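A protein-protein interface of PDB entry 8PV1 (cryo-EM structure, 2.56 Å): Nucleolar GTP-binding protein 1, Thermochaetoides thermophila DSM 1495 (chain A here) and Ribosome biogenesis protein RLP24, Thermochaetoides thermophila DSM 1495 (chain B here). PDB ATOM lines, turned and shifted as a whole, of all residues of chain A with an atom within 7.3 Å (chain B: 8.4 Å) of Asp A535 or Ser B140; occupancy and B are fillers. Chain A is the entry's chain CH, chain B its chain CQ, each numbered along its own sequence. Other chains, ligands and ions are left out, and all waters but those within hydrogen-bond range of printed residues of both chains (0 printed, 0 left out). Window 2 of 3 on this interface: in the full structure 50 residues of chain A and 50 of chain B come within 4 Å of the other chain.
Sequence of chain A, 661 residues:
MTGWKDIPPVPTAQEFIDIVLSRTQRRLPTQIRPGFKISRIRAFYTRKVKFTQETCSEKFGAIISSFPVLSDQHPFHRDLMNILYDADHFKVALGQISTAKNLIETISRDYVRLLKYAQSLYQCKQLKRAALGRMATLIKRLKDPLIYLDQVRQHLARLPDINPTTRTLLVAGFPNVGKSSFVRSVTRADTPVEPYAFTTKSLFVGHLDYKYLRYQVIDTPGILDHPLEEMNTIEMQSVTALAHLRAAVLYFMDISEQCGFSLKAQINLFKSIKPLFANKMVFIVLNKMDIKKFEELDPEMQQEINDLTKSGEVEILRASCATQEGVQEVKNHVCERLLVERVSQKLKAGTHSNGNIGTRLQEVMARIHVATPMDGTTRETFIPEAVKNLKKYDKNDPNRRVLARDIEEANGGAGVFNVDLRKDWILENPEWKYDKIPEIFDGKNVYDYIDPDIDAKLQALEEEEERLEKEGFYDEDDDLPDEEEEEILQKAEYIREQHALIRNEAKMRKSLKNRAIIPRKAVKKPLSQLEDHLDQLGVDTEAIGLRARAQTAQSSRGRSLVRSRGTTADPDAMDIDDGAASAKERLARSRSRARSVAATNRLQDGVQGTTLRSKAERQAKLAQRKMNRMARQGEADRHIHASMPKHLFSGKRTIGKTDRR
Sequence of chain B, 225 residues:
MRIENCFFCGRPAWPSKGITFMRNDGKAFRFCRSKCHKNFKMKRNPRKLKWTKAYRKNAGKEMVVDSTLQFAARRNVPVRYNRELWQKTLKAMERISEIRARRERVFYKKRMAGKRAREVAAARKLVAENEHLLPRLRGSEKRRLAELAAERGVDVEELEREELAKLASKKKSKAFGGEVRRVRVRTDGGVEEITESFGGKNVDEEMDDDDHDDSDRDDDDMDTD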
ATOM      1  N   GLN A 529      -9.150  -6.514 -24.155  1.00  0.00           N
ATOM      2  CA  GLN A 529      -9.942  -6.232 -22.962  1.00  0.00           C
ATOM      3  C   GLN A 529     -10.696  -4.912 -23.086  1.00  0.00           C
ATOM      4  O   GLN A 529     -11.857  -4.816 -22.669  1.00  0.00           O
ATOM      5  CB  GLN A 529      -9.048  -6.236 -21.724  1.00  0.00           C
ATOM      6  CG  GLN A 529      -8.239  -7.511 -21.564  1.00  0.00           C
ATOM      7  CD  GLN A 529      -7.826  -7.763 -20.129  1.00  0.00           C
ATOM      8  OE1 GLN A 529      -7.996  -6.905 -19.263  1.00  0.00           O
ATOM      9  NE2 GLN A 529      -7.284  -8.946 -19.867  1.00  0.00           N
ATOM     10  N   LEU A 530     -10.057  -3.887 -23.660  1.00  0.00           N
ATOM     11  CA  LEU A 530     -10.764  -2.633 -23.924  1.00  0.00           C
ATOM     12  C   LEU A 530     -11.900  -2.842 -24.921  1.00  0.00           C
ATOM     13  O   LEU A 530     -13.001  -2.296 -24.753  1.00  0.00           O
ATOM     14  CB  LEU A 530      -9.786  -1.575 -24.433  1.00  0.00           C
ATOM     15  CG  LEU A 530     -10.380  -0.205 -24.769  1.00  0.00           C
ATOM     16  CD1 LEU A 530     -11.173   0.368 -23.605  1.00  0.00           C
ATOM     17  CD2 LEU A 530      -9.286   0.756 -25.191  1.00  0.00           C
ATOM     18  N   GLU A 531     -11.639  -3.642 -25.962  1.00  0.00           N
ATOM     19  CA  GLU A 531     -12.650  -4.025 -26.942  1.00  0.00           C
ATOM     20  C   GLU A 531     -13.847  -4.677 -26.269  1.00  0.00           C
ATOM     21  O   GLU A 531     -14.995  -4.276 -26.495  1.00  0.00           O
ATOM     22  CB  GLU A 531     -12.017  -4.991 -27.949  1.00  0.00           C
ATOM     23  CG  GLU A 531     -12.909  -5.475 -29.080  1.00  0.00           C
ATOM     24  CD  GLU A 531     -13.329  -4.373 -30.023  1.00  0.00           C
ATOM     25  OE1 GLU A 531     -12.600  -3.366 -30.136  1.00  0.00           O
ATOM     26  OE2 GLU A 531     -14.393  -4.515 -30.662  1.00  0.00           O
ATOM     27  N   ASP A 532     -13.585  -5.660 -25.406  1.00  0.00           N
ATOM     28  CA  ASP A 532     -14.648  -6.395 -24.733  1.00  0.00           C
ATOM     29  C   ASP A 532     -15.449  -5.480 -23.814  1.00  0.00           C
ATOM     30  O   ASP A 532     -16.685  -5.508 -23.823  1.00  0.00           O
ATOM     31  CB  ASP A 532     -14.039  -7.565 -23.952  1.00  0.00           C
ATOM     32  CG  ASP A 532     -15.081  -8.531 -23.385  1.00  0.00           C
ATOM     33  OD1 ASP A 532     -16.302  -8.321 -23.549  1.00  0.00           O
ATOM     34  OD2 ASP A 532     -14.661  -9.524 -22.756  1.00  0.00           O
ATOM     35  N   HIS A 533     -14.762  -4.645 -23.026  1.00  0.00           N
ATOM     36  CA  HIS A 533     -15.465  -3.818 -22.049  1.00  0.00           C
ATOM     37  C   HIS A 533     -16.331  -2.767 -22.735  1.00  0.00           C
ATOM     38  O   HIS A 533     -17.493  -2.567 -22.360  1.00  0.00           O
ATOM     39  CB  HIS A 533     -14.476  -3.154 -21.093  1.00  0.00           C
ATOM     40  CG  HIS A 533     -15.134  -2.306 -20.050  1.00  0.00           C
ATOM     41  ND1 HIS A 533     -15.652  -2.829 -18.885  1.00  0.00           N
ATOM     42  CD2 HIS A 533     -15.389  -0.977 -20.010  1.00  0.00           C
ATOM     43  CE1 HIS A 533     -16.180  -1.856 -18.164  1.00  0.00           C
ATOM     44  NE2 HIS A 533     -16.031  -0.722 -18.824  1.00  0.00           N
ATOM     45  N   LEU A 534     -15.793  -2.107 -23.766  1.00  0.00           N
ATOM     46  CA  LEU A 534     -16.591  -1.132 -24.503  1.00  0.00           C
ATOM     47  C   LEU A 534     -17.728  -1.809 -25.260  1.00  0.00           C
ATOM     48  O   LEU A 534     -18.807  -1.225 -25.429  1.00  0.00           O
ATOM     49  CB  LEU A 534     -15.701  -0.344 -25.463  1.00  0.00           C
ATOM     50  CG  LEU A 534     -14.752   0.671 -24.826  1.00  0.00           C
ATOM     51  CD1 LEU A 534     -13.996   1.429 -25.897  1.00  0.00           C
ATOM     52  CD2 LEU A 534     -15.516   1.632 -23.936  1.00  0.00           C
ATOM     53  N   ASP A 535     -17.510  -3.050 -25.704  1.00  0.00           N
ATOM     54  CA  ASP A 535     -18.537  -3.766 -26.448  1.00  0.00           C
ATOM     55  C   ASP A 535     -19.718  -4.102 -25.537  1.00  0.00           C
ATOM     56  O   ASP A 535     -20.879  -3.924 -25.921  1.00  0.00           O
ATOM     57  CB  ASP A 535     -17.915  -5.021 -27.072  1.00  0.00           C
ATOM     58  CG  ASP A 535     -18.835  -5.726 -28.062  1.00  0.00           C
ATOM     59  OD1 ASP A 535     -19.979  -5.283 -28.270  1.00  0.00           O
ATOM     60  OD2 ASP A 535     -18.391  -6.728 -28.663  1.00  0.00           O
ATOM     61  N   GLN A 536     -19.441  -4.570 -24.312  1.00  0.00           N
ATOM     62  CA  GLN A 536     -20.531  -4.751 -23.349  1.00  0.00           C
ATOM     63  C   GLN A 536     -21.158  -3.432 -22.918  1.00  0.00           C
ATOM     64  O   GLN A 536     -22.362  -3.401 -22.641  1.00  0.00           O
ATOM     65  CB  GLN A 536     -20.093  -5.510 -22.092  1.00  0.00           C
ATOM     66  CG  GLN A 536     -19.150  -6.668 -22.280  1.00  0.00           C
ATOM     67  CD  GLN A 536     -19.341  -7.730 -21.215  1.00  0.00           C
ATOM     68  OE1 GLN A 536     -20.255  -7.643 -20.396  1.00  0.00           O
ATOM     69  NE2 GLN A 536     -18.471  -8.732 -21.215  1.00  0.00           N
ATOM     70  N   LEU A 537     -20.387  -2.346 -22.851  1.00  0.00           N
ATOM     71  CA  LEU A 537     -20.977  -1.042 -22.569  1.00  0.00           C
ATOM     72  C   LEU A 537     -21.834  -0.518 -23.712  1.00  0.00           C
ATOM     73  O   LEU A 537     -22.606   0.424 -23.506  1.00  0.00           O
ATOM     74  CB  LEU A 537     -19.895  -0.011 -22.237  1.00  0.00           C
ATOM     75  CG  LEU A 537     -19.158  -0.162 -20.908  1.00  0.00           C
ATOM     76  CD1 LEU A 537     -18.259   1.037 -20.680  1.00  0.00           C
ATOM     77  CD2 LEU A 537     -20.141  -0.329 -19.763  1.00  0.00           C
ATOM     78  N   GLY A 538     -21.719  -1.094 -24.905  1.00  0.00           N
ATOM     79  CA  GLY A 538     -22.631  -0.750 -25.976  1.00  0.00           C
ATOM     80  C   GLY A 538     -22.075   0.227 -26.979  1.00  0.00           C
ATOM     81  O   GLY A 538     -22.822   1.049 -27.517  1.00  0.00           O
ATOM     82  N   VAL A 539     -20.782   0.158 -27.247  1.00  0.00           N
ATOM     83  CA  VAL A 539     -20.118   1.039 -28.194  1.00  0.00           C
ATOM     84  C   VAL A 539     -19.689   0.217 -29.398  1.00  0.00           C
ATOM     85  O   VAL A 539     -19.049  -0.832 -29.253  1.00  0.00           O
ATOM     86  CB  VAL A 539     -18.913   1.743 -27.541  1.00  0.00           C
ATOM     87  CG1 VAL A 539     -18.247   2.684 -28.527  1.00  0.00           C
ATOM     88  CG2 VAL A 539     -19.351   2.494 -26.296  1.00  0.00           C
ATOM     89  N   ASP A 540     -20.057   0.681 -30.587  1.00  0.00           N
ATOM     90  CA  ASP A 540     -19.633   0.038 -31.827  1.00  0.00           C
ATOM     91  C   ASP A 540     -18.192   0.449 -32.087  1.00  0.00           C
ATOM     92  O   ASP A 540     -17.922   1.527 -32.624  1.00  0.00           O
ATOM     93  CB  ASP A 540     -20.553   0.425 -32.979  1.00  0.00           C
ATOM     94  CG  ASP A 540     -20.490  -0.561 -34.125  1.00  0.00           C
ATOM     95  OD1 ASP A 540     -20.669  -1.773 -33.885  1.00  0.00           O
ATOM     96  OD2 ASP A 540     -20.262  -0.121 -35.270  1.00  0.00           O
ATOM     97  N   THR A 541     -17.258  -0.420 -31.698  1.00  0.00           N
ATOM     98  CA  THR A 541     -15.844  -0.069 -31.742  1.00  0.00           C
ATOM     99  C   THR A 541     -15.308  -0.089 -33.167  1.00  0.00           C
ATOM    100  O   THR A 541     -14.268   0.514 -33.456  1.00  0.00           O
ATOM    101  CB  THR A 541     -15.048  -1.030 -30.867  1.00  0.00           C
ATOM    102  OG1 THR A 541     -15.078  -2.334 -31.457  1.00  0.00           O
ATOM    103  CG2 THR A 541     -15.652  -1.099 -29.479  1.00  0.00           C
ATOM    104  N   GLU A 542     -15.999  -0.786 -34.070  1.00  0.00           N
ATOM    105  CA  GLU A 542     -15.557  -0.830 -35.458  1.00  0.00           C
ATOM    106  C   GLU A 542     -15.791   0.505 -36.151  1.00  0.00           C
ATOM    107  O   GLU A 542     -15.073   0.858 -37.094  1.00  0.00           O
ATOM    108  CB  GLU A 542     -16.270  -1.960 -36.196  1.00  0.00           C
ATOM    109  CG  GLU A 542     -16.174  -3.296 -35.486  1.00  0.00           C
ATOM    110  CD  GLU A 542     -15.074  -4.175 -36.044  1.00  0.00           C
ATOM    111  OE1 GLU A 542     -14.913  -5.310 -35.550  1.00  0.00           O
ATOM    112  OE2 GLU A 542     -14.372  -3.731 -36.977  1.00  0.00           O
ATOM    113  N   ARG B 136     -28.358  -4.374 -21.514  1.00  0.00           N
ATOM    114  CA  ARG B 136     -28.340  -3.812 -22.854  1.00  0.00           C
ATOM    115  C   ARG B 136     -27.595  -4.773 -23.767  1.00  0.00           C
ATOM    116  O   ARG B 136     -26.838  -5.633 -23.309  1.00  0.00           O
ATOM    117  CB  ARG B 136     -27.670  -2.433 -22.881  1.00  0.00           C
ATOM    118  CG  ARG B 136     -26.198  -2.469 -22.503  1.00  0.00           C
ATOM    119  CD  ARG B 136     -25.586  -1.081 -22.418  1.00  0.00           C
ATOM    120  NE  ARG B 136     -26.017  -0.358 -21.229  1.00  0.00           N
ATOM    121  CZ  ARG B 136     -25.967   0.960 -21.097  1.00  0.00           C
ATOM    122  NH1 ARG B 136     -25.509   1.734 -22.066  1.00  0.00           N
ATOM    123  NH2 ARG B 136     -26.380   1.515 -19.961  1.00  0.00           N
ATOM    124  N   LEU B 137     -27.811  -4.618 -25.066  1.00  0.00           N
ATOM    125  CA  LEU B 137     -27.166  -5.484 -26.039  1.00  0.00           C
ATOM    126  C   LEU B 137     -25.818  -4.915 -26.458  1.00  0.00           C
ATOM    127  O   LEU B 137     -25.586  -3.705 -26.405  1.00  0.00           O
ATOM    128  CB  LEU B 137     -28.058  -5.685 -27.263  1.00  0.00           C
ATOM    129  CG  LEU B 137     -29.309  -6.513 -26.975  1.00  0.00           C
ATOM    130  CD1 LEU B 137     -30.176  -6.634 -28.212  1.00  0.00           C
ATOM    131  CD2 LEU B 137     -28.942  -7.885 -26.426  1.00  0.00           C
ATOM    132  N   ARG B 138     -24.931  -5.812 -26.876  1.00  0.00           N
ATOM    133  CA  ARG B 138     -23.581  -5.436 -27.263  1.00  0.00           C
ATOM    134  C   ARG B 138     -23.596  -4.644 -28.568  1.00  0.00           C
ATOM    135  O   ARG B 138     -24.569  -4.672 -29.324  1.00  0.00           O
ATOM    136  CB  ARG B 138     -22.722  -6.689 -27.421  1.00  0.00           C
ATOM    137  CG  ARG B 138     -22.335  -7.357 -26.115  1.00  0.00           C
ATOM    138  CD  ARG B 138     -21.811  -8.755 -26.373  1.00  0.00           C
ATOM    139  NE  ARG B 138     -21.130  -9.314 -25.213  1.00  0.00           N
ATOM    140  CZ  ARG B 138     -19.819  -9.283 -25.021  1.00  0.00           C
ATOM    141  NH1 ARG B 138     -19.007  -8.695 -25.883  1.00  0.00           N
ATOM    142  NH2 ARG B 138     -19.310  -9.860 -23.936  1.00  0.00           N
ATOM    143  N   GLY B 139     -22.502  -3.921 -28.823  1.00  0.00           N
ATOM    144  CA  GLY B 139     -22.403  -3.155 -30.058  1.00  0.00           C
ATOM    145  C   GLY B 139     -22.330  -4.034 -31.293  1.00  0.00           C
ATOM    146  O   GLY B 139     -22.955  -3.739 -32.317  1.00  0.00           O
ATOM    147  N   SER B 140     -21.570  -5.129 -31.213  1.00  0.00           N
ATOM    148  CA  SER B 140     -21.520  -6.083 -32.316  1.00  0.00           C
ATOM    149  C   SER B 140     -22.870  -6.762 -32.517  1.00  0.00           C
ATOM    150  O   SER B 140     -23.271  -7.039 -33.655  1.00  0.00           O
ATOM    151  CB  SER B 140     -20.428  -7.119 -32.062  1.00  0.00           C
ATOM    152  OG  SER B 140     -20.646  -7.798 -30.839  1.00  0.00           O
ATOM    153  N   GLU B 141     -23.583  -7.035 -31.421  1.00  0.00           N
ATOM    154  CA  GLU B 141     -24.931  -7.586 -31.522  1.00  0.00           C
ATOM    155  C   GLU B 141     -25.879  -6.603 -32.198  1.00  0.00           C
ATOM    156  O   GLU B 141     -26.713  -7.000 -33.018  1.00  0.00           O
ATOM    157  CB  GLU B 141     -25.448  -7.969 -30.134  1.00  0.00           C
ATOM    158  CG  GLU B 141     -24.693  -9.115 -29.479  1.00  0.00           C
ATOM    159  CD  GLU B 141     -24.881 -10.433 -30.207  1.00  0.00           C
ATOM    160  OE1 GLU B 141     -25.966 -10.645 -30.789  1.00  0.00           O
ATOM    161  OE2 GLU B 141     -23.944 -11.259 -30.197  1.00  0.00           O
ATOM    162  N   LYS B 142     -25.759  -5.312 -31.871  1.00  0.00           N
ATOM    163  CA  LYS B 142     -26.577  -4.298 -32.531  1.00  0.00           C
ATOM    164  C   LYS B 142     -26.256  -4.205 -34.018  1.00  0.00           C
ATOM    165  O   LYS B 142     -27.164  -4.068 -34.845  1.00  0.00           O
ATOM    166  CB  LYS B 142     -26.381  -2.937 -31.864  1.00  0.00           C
ATOM    167  CG  LYS B 142     -27.002  -2.812 -30.487  1.00  0.00           C
ATOM    168  CD  LYS B 142     -27.064  -1.358 -30.053  1.00  0.00           C
ATOM    169  CE  LYS B 142     -27.631  -1.218 -28.651  1.00  0.00           C
ATOM    170  NZ  LYS B 142     -26.690  -1.730 -27.617  1.00  0.00           N
ATOM    171  N   ARG B 143     -24.970  -4.285 -34.374  1.00  0.00           N
ATOM    172  CA  ARG B 143     -24.578  -4.259 -35.782  1.00  0.00           C
ATOM    173  C   ARG B 143     -25.131  -5.464 -36.540  1.00  0.00           C
ATOM    174  O   ARG B 143     -25.658  -5.326 -37.654  1.00  0.00           O
ATOM    175  CB  ARG B 143     -23.055  -4.202 -35.901  1.00  0.00           C
ATOM    176  CG  ARG B 143     -22.561  -3.555 -37.185  1.00  0.00           C
ATOM    177  CD  ARG B 143     -22.374  -2.054 -37.042  1.00  0.00           C
ATOM    178  NE  ARG B 143     -21.616  -1.504 -38.158  1.00  0.00           N
ATOM    179  CZ  ARG B 143     -21.188  -0.251 -38.232  1.00  0.00           C
ATOM    180  NH1 ARG B 143     -21.428   0.620 -37.266  1.00  0.00           N
ATOM    181  NH2 ARG B 143     -20.500   0.137 -39.303  1.00  0.00           N
ATOM    182  N   ARG B 144     -25.034  -6.655 -35.942  1.00  0.00           N
ATOM    183  CA  ARG B 144     -25.508  -7.851 -36.629  1.00  0.00           C
ATOM    184  C   ARG B 144     -27.034  -7.873 -36.709  1.00  0.00           C
ATOM    185  O   ARG B 144     -27.599  -8.334 -37.707  1.00  0.00           O
ATOM    186  CB  ARG B 144     -24.946  -9.112 -35.961  1.00  0.00           C
ATOM    187  CG  ARG B 144     -25.710  -9.667 -34.770  1.00  0.00           C
ATOM    188  CD  ARG B 144     -25.459 -11.157 -34.613  1.00  0.00           C
ATOM    189  NE  ARG B 144     -26.405 -11.779 -33.695  1.00  0.00           N
ATOM    190  CZ  ARG B 144     -26.447 -13.077 -33.428  1.00  0.00           C
ATOM    191  NH1 ARG B 144     -25.603 -13.925 -33.992  1.00  0.00           N
ATOM    192  NH2 ARG B 144     -27.357 -13.535 -32.573  1.00  0.00           N
ATOM    193  N   LEU B 145     -27.719  -7.319 -35.704  1.00  0.00           N
ATOM    194  CA  LEU B 145     -29.172  -7.228 -35.780  1.00  0.00           C
ATOM    195  C   LEU B 145     -29.605  -6.200 -36.816  1.00  0.00           C
ATOM    196  O   LEU B 145     -30.611  -6.396 -37.506  1.00  0.00           O
ATOM    197  CB  LEU B 145     -29.761  -6.895 -34.410  1.00  0.00           C
ATOM    198  CG  LEU B 145     -29.800  -8.041 -33.396  1.00  0.00           C
ATOM    199  CD1 LEU B 145     -30.546  -7.619 -32.144  1.00  0.00           C
ATOM    200  CD2 LEU B 145     -30.430  -9.282 -34.006  1.00  0.00           C
ATOM    201  N   ALA B 146     -28.848  -5.108 -36.951  1.00  0.00           N
ATOM    202  CA  ALA B 146     -29.156  -4.110 -37.971  1.00  0.00           C
ATOM    203  C   ALA B 146     -28.984  -4.682 -39.372  1.00  0.00           C
ATOM    204  O   ALA B 146     -29.824  -4.458 -40.253  1.00  0.00           O
ATOM    205  CB  ALA B 146     -28.277  -2.875 -37.777  1.00  0.00           C
ATOM    206  N   GLU B 147     -27.908  -5.445 -39.597  1.00  0.00           N
ATOM    207  CA  GLU B 147     -27.710  -6.009 -40.931  1.00  0.00           C
ATOM    208  C   GLU B 147     -28.700  -7.139 -41.212  1.00  0.00           C
ATOM    209  O   GLU B 147     -29.143  -7.304 -42.355  1.00  0.00           O
ATOM    210  CB  GLU B 147     -26.259  -6.465 -41.124  1.00  0.00           C
ATOM    211  CG  GLU B 147     -25.793  -7.639 -40.285  1.00  0.00           C
ATOM    212  CD  GLU B 147     -25.961  -8.971 -40.990  1.00  0.00           C
ATOM    213  OE1 GLU B 147     -26.078  -8.978 -42.233  1.00  0.00           O
ATOM    214  OE2 GLU B 147     -25.976 -10.013 -40.299  1.00  0.00           O
ATOM    215  N   GLU B 160     -34.166  -6.443 -31.600  1.00  0.00           N
ATOM    216  CA  GLU B 160     -33.521  -6.019 -30.357  1.00  0.00           C
ATOM    217  C   GLU B 160     -34.241  -6.576 -29.136  1.00  0.00           C
ATOM    218  O   GLU B 160     -33.601  -7.075 -28.203  1.00  0.00           O
ATOM    219  CB  GLU B 160     -33.455  -4.491 -30.272  1.00  0.00           C
ATOM    220  CG  GLU B 160     -32.613  -3.807 -31.334  1.00  0.00           C
ATOM    221  CD  GLU B 160     -31.129  -4.018 -31.136  1.00  0.00           C
ATOM    222  OE1 GLU B 160     -30.665  -3.907 -29.983  1.00  0.00           O
ATOM    223  OE2 GLU B 160     -30.426  -4.282 -32.134  1.00  0.00           O
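NH1 of Arg B136 lies within hydrogen-bond range of O of Leu A537 (3.5 Å).
The guanidinium group (NH2) of Arg B138 is in salt-bridge range of the side-chain carboxylate (OD1) of Asp A532 (3.4 Å).
The guanidinium group (NH1) of Arg B138 is in salt-bridge range of the side-chain carboxylate (OD2) of Asp A535, 3.5 Å away.
The guanidinium group (NH2) of Arg B138 lies close to the side-chain amide nitrogen (NE2) of Gln A536 (3.1 Å).
The side-chain carboxylate of Asp A535 lies within hydrogen-bond range of the backbone NH of Gly B139 (2.9 Å).
The side-chain hydroxyl (OG) of Ser B140 lies within hydrogen-bond range of the side-chain carboxylate (OD2) of Asp A535 (3.3 Å).
The side-chain carboxylate (OD2) of Asp A540 is in salt-bridge range of the guanidinium group (NH1) of Arg B143, at 2.4 Å.
The side-chain carboxylate of Asp A540 lies close to the backbone carbonyl oxygen of Gly B139, at 3.4 Å.
The side-chain carboxylate (OD1) of Asp A532 is in hydrogen-bond range of the side-chain amide nitrogen (NE2) of Gln A536 (3.2 Å).
Among the printed residues, pairs that only touch across the chains: Gln A536 with Arg B136.
Of the printed residues of chain B, Leu A537 touches Arg B136.
Of the printed residues of chain A, Arg B136 touches Gln A536 and Leu A537.
Of the printed residues of chain A, Arg B138 touches Asp A532, Asp A535 and Gln A536.
Gly B139 touches two residues of chain A.
Ser B140 touches one residue of chain A.
Printed residues of chain A within 4 Å of Arg B143: Asp A540 (2.4 Å).
Glu B160 touches none of the printed residues of chain A.
The nearest residue of chain B that does not touch Asp A535 is Leu B137 (4.7 Å).
The nearest residue of chain A that does not touch Ser B140 is Asp A540 (4.4 Å).
The nearest printed residue of chain B that does not touch Asp A540 is Ser B140 (4.4 Å).
Printed residues of chain A that touch a printed residue of chain B: Asp A532, Asp A535, Gln A536, Leu A537 and Asp A540.
Printed residues of chain B that touch a printed residue of chain A: Arg B136, Arg B138, Gly B139, Ser B140 and Arg B143.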
